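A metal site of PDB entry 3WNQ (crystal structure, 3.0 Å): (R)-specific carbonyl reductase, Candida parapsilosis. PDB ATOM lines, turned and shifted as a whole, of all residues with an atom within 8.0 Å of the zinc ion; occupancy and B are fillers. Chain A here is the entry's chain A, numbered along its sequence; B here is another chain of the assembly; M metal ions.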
ATOM      1  N   ASN A  98       6.426  27.588  20.131  1.00  0.00           N
ATOM      2  CA  ASN A  98       7.122  27.454  21.421  1.00  0.00           C
ATOM      3  C   ASN A  98       7.786  26.115  21.532  1.00  0.00           C
ATOM      4  O   ASN A  98       7.705  25.494  22.564  1.00  0.00           O
ATOM      5  CB  ASN A  98       6.118  27.609  22.579  1.00  0.00           C
ATOM      6  CG  ASN A  98       6.771  27.908  23.946  1.00  0.00           C
ATOM      7  OD1 ASN A  98       7.964  28.204  24.068  1.00  0.00           O
ATOM      8  ND2 ASN A  98       5.971  27.854  24.965  1.00  0.00           N
ATOM      9  N   GLY A  99       8.443  25.651  20.482  1.00  0.00           N
ATOM     10  CA  GLY A  99       9.083  24.347  20.569  1.00  0.00           C
ATOM     11  C   GLY A  99       9.729  24.024  21.918  1.00  0.00           C
ATOM     12  O   GLY A  99      10.160  24.926  22.638  1.00  0.00           O
ATOM     13  N   CYS A 100       9.827  22.733  22.256  1.00  0.00           N
ATOM     14  CA  CYS A 100      10.417  22.270  23.533  1.00  0.00           C
ATOM     15  C   CYS A 100      11.924  22.448  23.669  1.00  0.00           C
ATOM     16  O   CYS A 100      12.432  22.375  24.774  1.00  0.00           O
ATOM     17  CB  CYS A 100      10.105  20.781  23.767  1.00  0.00           C
ATOM     18  SG  CYS A 100      11.287  19.622  23.080  1.00  0.00           S
ATOM     19  N   GLY A 101      12.614  22.646  22.554  1.00  0.00           N
ATOM     20  CA  GLY A 101      14.045  22.880  22.534  1.00  0.00           C
ATOM     21  C   GLY A 101      14.963  21.766  22.974  1.00  0.00           C
ATOM     22  O   GLY A 101      16.183  22.007  23.130  1.00  0.00           O
ATOM     23  N   GLY A 102      14.391  20.563  23.145  1.00  0.00           N
ATOM     24  CA  GLY A 102      15.168  19.419  23.576  1.00  0.00           C
ATOM     25  C   GLY A 102      14.910  18.093  22.873  1.00  0.00           C
ATOM     26  O   GLY A 102      15.538  17.106  23.217  1.00  0.00           O
ATOM     27  N   CYS A 103      14.012  18.054  21.897  1.00  0.00           N
ATOM     28  CA  CYS A 103      13.756  16.796  21.198  1.00  0.00           C
ATOM     29  C   CYS A 103      14.426  16.729  19.843  1.00  0.00           C
ATOM     30  O   CYS A 103      14.977  17.714  19.392  1.00  0.00           O
ATOM     31  CB  CYS A 103      12.259  16.582  20.994  1.00  0.00           C
ATOM     32  SG  CYS A 103      11.495  17.643  19.847  1.00  0.00           S
ATOM     33  N   LYS A 104      14.360  15.567  19.174  1.00  0.00           N
ATOM     34  CA  LYS A 104      14.985  15.434  17.851  1.00  0.00           C
ATOM     35  C   LYS A 104      14.492  16.471  16.834  1.00  0.00           C
ATOM     36  O   LYS A 104      15.273  16.922  16.021  1.00  0.00           O
ATOM     37  CB  LYS A 104      14.840  13.999  17.273  1.00  0.00           C
ATOM     38  CG  LYS A 104      13.621  13.643  16.399  1.00  0.00           C
ATOM     39  CD  LYS A 104      13.634  12.110  16.064  1.00  0.00           C
ATOM     40  CE  LYS A 104      12.636  11.649  14.970  1.00  0.00           C
ATOM     41  NZ  LYS A 104      13.231  11.414  13.598  1.00  0.00           N
ATOM     42  N   TYR A 105      13.233  16.897  16.902  1.00  0.00           N
ATOM     43  CA  TYR A 105      12.787  17.901  15.939  1.00  0.00           C
ATOM     44  C   TYR A 105      13.364  19.301  16.253  1.00  0.00           C
ATOM     45  O   TYR A 105      13.865  19.962  15.337  1.00  0.00           O
ATOM     46  CB  TYR A 105      11.247  17.946  15.835  1.00  0.00           C
ATOM     47  CG  TYR A 105      10.647  16.600  15.473  1.00  0.00           C
ATOM     48  CD1 TYR A 105      10.466  16.199  14.156  1.00  0.00           C
ATOM     49  CD2 TYR A 105      10.350  15.671  16.477  1.00  0.00           C
ATOM     50  CE1 TYR A 105      10.029  14.885  13.833  1.00  0.00           C
ATOM     51  CE2 TYR A 105       9.909  14.361  16.197  1.00  0.00           C
ATOM     52  CZ  TYR A 105       9.760  13.967  14.875  1.00  0.00           C
ATOM     53  OH  TYR A 105       9.384  12.631  14.655  1.00  0.00           O
ATOM     54  N   CYS A 106      13.352  19.756  17.510  1.00  0.00           N
ATOM     55  CA  CYS A 106      13.863  21.101  17.812  1.00  0.00           C
ATOM     56  C   CYS A 106      15.362  21.228  17.574  1.00  0.00           C
ATOM     57  O   CYS A 106      15.852  22.229  17.027  1.00  0.00           O
ATOM     58  CB  CYS A 106      13.560  21.461  19.246  1.00  0.00           C
ATOM     59  SG  CYS A 106      11.842  21.457  19.614  1.00  0.00           S
ATOM     60  N   ARG A 107      16.080  20.185  17.995  1.00  0.00           N
ATOM     61  CA  ARG A 107      17.520  20.129  17.873  1.00  0.00           C
ATOM     62  C   ARG A 107      17.874  20.035  16.407  1.00  0.00           C
ATOM     63  O   ARG A 107      18.987  20.389  16.007  1.00  0.00           O
ATOM     64  CB  ARG A 107      18.070  18.902  18.613  1.00  0.00           C
ATOM     65  CG  ARG A 107      17.662  18.816  20.040  1.00  0.00           C
ATOM     66  CD  ARG A 107      18.771  18.199  20.826  1.00  0.00           C
ATOM     67  NE  ARG A 107      18.480  16.938  21.533  1.00  0.00           N
ATOM     68  CZ  ARG A 107      18.317  15.742  20.960  1.00  0.00           C
ATOM     69  NH1 ARG A 107      18.382  15.616  19.645  1.00  0.00           N
ATOM     70  NH2 ARG A 107      18.124  14.646  21.723  1.00  0.00           N
ATOM     71  N   GLY A 108      16.910  19.557  15.631  1.00  0.00           N
ATOM     72  CA  GLY A 108      17.098  19.396  14.201  1.00  0.00           C
ATOM     73  C   GLY A 108      16.583  20.500  13.292  1.00  0.00           C
ATOM     74  O   GLY A 108      16.371  20.284  12.105  1.00  0.00           O
ATOM     75  N   ILE A 110      13.641  22.079  13.232  1.00  0.00           N
ATOM     76  CA  ILE A 110      12.228  22.128  12.968  1.00  0.00           C
ATOM     77  C   ILE A 110      11.422  22.123  14.267  1.00  0.00           C
ATOM     78  O   ILE A 110      10.656  21.208  14.539  1.00  0.00           O
ATOM     79  CB  ILE A 110      11.763  21.013  11.970  1.00  0.00           C
ATOM     80  CG1 ILE A 110      12.447  19.705  12.229  1.00  0.00           C
ATOM     81  CG2 ILE A 110      12.056  21.469  10.562  1.00  0.00           C
ATOM     82  CD1 ILE A 110      11.834  18.589  11.457  1.00  0.00           C
ATOM     83  N   ASP A 111      11.612  23.159  15.073  1.00  0.00           N
ATOM     84  CA  ASP A 111      10.897  23.273  16.321  1.00  0.00           C
ATOM     85  C   ASP A 111       9.394  23.558  16.121  1.00  0.00           C
ATOM     86  O   ASP A 111       8.590  23.449  17.067  1.00  0.00           O
ATOM     87  CB  ASP A 111      11.550  24.381  17.181  1.00  0.00           C
ATOM     88  CG  ASP A 111      11.865  25.668  16.406  1.00  0.00           C
ATOM     89  OD1 ASP A 111      10.944  26.392  15.961  1.00  0.00           O
ATOM     90  OD2 ASP A 111      13.065  25.931  16.263  1.00  0.00           O
ATOM     91  N   ASN A 112       9.017  23.882  14.884  1.00  0.00           N
ATOM     92  CA  ASN A 112       7.637  24.179  14.598  1.00  0.00           C
ATOM     93  C   ASN A 112       6.792  22.929  14.538  1.00  0.00           C
ATOM     94  O   ASN A 112       5.550  22.993  14.510  1.00  0.00           O
ATOM     95  CB  ASN A 112       7.505  24.945  13.280  1.00  0.00           C
ATOM     96  CG  ASN A 112       7.902  24.126  12.040  1.00  0.00           C
ATOM     97  OD1 ASN A 112       8.900  23.390  12.018  1.00  0.00           O
ATOM     98  ND2 ASN A 112       7.137  24.299  10.964  1.00  0.00           N
ATOM     99  N   VAL A 113       7.439  21.780  14.561  1.00  0.00           N
ATOM    100  CA  VAL A 113       6.664  20.558  14.531  1.00  0.00           C
ATOM    101  C   VAL A 113       6.851  19.693  15.768  1.00  0.00           C
ATOM    102  O   VAL A 113       6.372  18.530  15.781  1.00  0.00           O
ATOM    103  CB  VAL A 113       6.978  19.708  13.273  1.00  0.00           C
ATOM    104  CG1 VAL A 113       6.552  20.439  12.090  1.00  0.00           C
ATOM    105  CG2 VAL A 113       8.390  19.408  13.190  1.00  0.00           C
ATOM    106  N   CYS A 114       7.525  20.261  16.786  1.00  0.00           N
ATOM    107  CA  CYS A 114       7.822  19.600  18.072  1.00  0.00           C
ATOM    108  C   CYS A 114       6.595  18.870  18.630  1.00  0.00           C
ATOM    109  O   CYS A 114       5.546  19.471  18.902  1.00  0.00           O
ATOM    110  CB  CYS A 114       8.330  20.632  19.081  1.00  0.00           C
ATOM    111  SG  CYS A 114       8.751  20.070  20.776  1.00  0.00           S
ATOM    112  N   LYS A 115       6.700  17.557  18.793  1.00  0.00           N
ATOM    113  CA  LYS A 115       5.570  16.809  19.302  1.00  0.00           C
ATOM    114  C   LYS A 115       5.292  17.198  20.735  1.00  0.00           C
ATOM    115  O   LYS A 115       4.132  17.288  21.143  1.00  0.00           O
ATOM    116  CB  LYS A 115       5.809  15.307  19.220  1.00  0.00           C
ATOM    117  CG  LYS A 115       5.768  14.744  17.852  1.00  0.00           C
ATOM    118  CD  LYS A 115       6.034  13.234  17.936  1.00  0.00           C
ATOM    119  CE  LYS A 115       6.241  12.567  16.536  1.00  0.00           C
ATOM    120  NZ  LYS A 115       7.182  11.389  16.621  1.00  0.00           N
ATOM    121  N   ASN A 116       6.366  17.472  21.490  1.00  0.00           N
ATOM    122  CA  ASN A 116       6.265  17.830  22.910  1.00  0.00           C
ATOM    123  C   ASN A 116       5.570  19.121  23.215  1.00  0.00           C
ATOM    124  O   ASN A 116       5.040  19.311  24.291  1.00  0.00           O
ATOM    125  CB  ASN A 116       7.648  17.921  23.515  1.00  0.00           C
ATOM    126  CG  ASN A 116       8.372  16.598  23.526  1.00  0.00           C
ATOM    127  OD1 ASN A 116       7.817  15.606  23.141  1.00  0.00           O
ATOM    128  ND2 ASN A 116       9.613  16.590  23.984  1.00  0.00           N
ATOM    129  N   ALA A 117       5.593  20.049  22.285  1.00  0.00           N
ATOM    130  CA  ALA A 117       5.002  21.357  22.520  1.00  0.00           C
ATOM    131  C   ALA A 117       3.569  21.485  22.111  1.00  0.00           C
ATOM    132  O   ALA A 117       3.020  22.584  22.131  1.00  0.00           O
ATOM    133  CB  ALA A 117       5.835  22.432  21.822  1.00  0.00           C
ATOM    134  N   ARG A 138      10.419  28.956  27.946  1.00  0.00           N
ATOM    135  CA  ARG A 138      11.620  28.627  27.152  1.00  0.00           C
ATOM    136  C   ARG A 138      12.056  29.792  26.281  1.00  0.00           C
ATOM    137  O   ARG A 138      11.473  30.059  25.232  1.00  0.00           O
ATOM    138  CB  ARG A 138      11.333  27.440  26.277  1.00  0.00           C
ATOM    139  CG  ARG A 138      11.015  26.237  27.084  1.00  0.00           C
ATOM    140  CD  ARG A 138      10.832  24.997  26.275  1.00  0.00           C
ATOM    141  NE  ARG A 138       9.570  25.023  25.593  1.00  0.00           N
ATOM    142  CZ  ARG A 138       8.350  24.792  26.078  1.00  0.00           C
ATOM    143  NH1 ARG A 138       7.359  24.894  25.229  1.00  0.00           N
ATOM    144  NH2 ARG A 138       8.061  24.456  27.325  1.00  0.00           N
ATOM    145  N   ARG A 140      14.330  30.095  24.309  1.00  0.00           N
ATOM    146  CA  ARG A 140      14.841  29.770  22.972  1.00  0.00           C
ATOM    147  C   ARG A 140      13.802  30.233  21.941  1.00  0.00           C
ATOM    148  O   ARG A 140      14.134  30.623  20.847  1.00  0.00           O
ATOM    149  CB  ARG A 140      15.133  28.250  22.812  1.00  0.00           C
ATOM    150  CG  ARG A 140      13.940  27.424  22.289  1.00  0.00           C
ATOM    151  CD  ARG A 140      14.248  25.933  22.154  1.00  0.00           C
ATOM    152  NE  ARG A 140      14.948  25.553  20.928  1.00  0.00           N
ATOM    153  CZ  ARG A 140      14.437  25.654  19.702  1.00  0.00           C
ATOM    154  NH1 ARG A 140      15.163  25.269  18.671  1.00  0.00           N
ATOM    155  NH2 ARG A 140      13.227  26.130  19.501  1.00  0.00           N
ATOM    156  N   ASN B  85      11.220  15.222  29.879  1.00  0.00           N
ATOM    157  CA  ASN B  85      11.700  14.271  28.874  1.00  0.00           C
ATOM    158  C   ASN B  85      12.567  13.181  29.489  1.00  0.00           C
ATOM    159  O   ASN B  85      12.719  12.114  28.903  1.00  0.00           O
ATOM    160  CB  ASN B  85      12.473  14.957  27.735  1.00  0.00           C
ATOM    161  CG  ASN B  85      11.747  16.189  27.197  1.00  0.00           C
ATOM    162  OD1 ASN B  85      10.502  16.264  27.204  1.00  0.00           O
ATOM    163  ND2 ASN B  85      12.518  17.160  26.722  1.00  0.00           N
HETATM  164 ZN    ZN M   1      10.976  19.610  20.717  1.00  0.00          ZN
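N of Gly 101 touches the zinc ion, at 3.9 Å. Of the 22 residues printed, 5 come within 4 Å of the zinc ion.
The backbone NH of Gly 102 sits close to the side-chain sulfur of Cys 100, at 3.2 Å. SG of Cys 100 lies close to ND2 of Asn 116, at 3.6 Å. N of Ala 117 sits close to SG of Cys 114, at 3.5 Å. The side-chain sulfur (SG) of Cys 106 lies close to the backbone NH (N) of Gly 101 (3.3 Å). The backbone NH (N) of Tyr 105 sits close to the side-chain sulfur (SG) of Cys 103 (3.5 Å). SG of Cys 114 sits close to N of Asn 116, at 3.6 Å.
The zinc ion is bound by SG of Cys 103 (2.2 Å), SG of Cys 114 (2.3 Å), SG of Cys 106 (2.3 Å) and SG of Cys 100 (2.4 Å).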
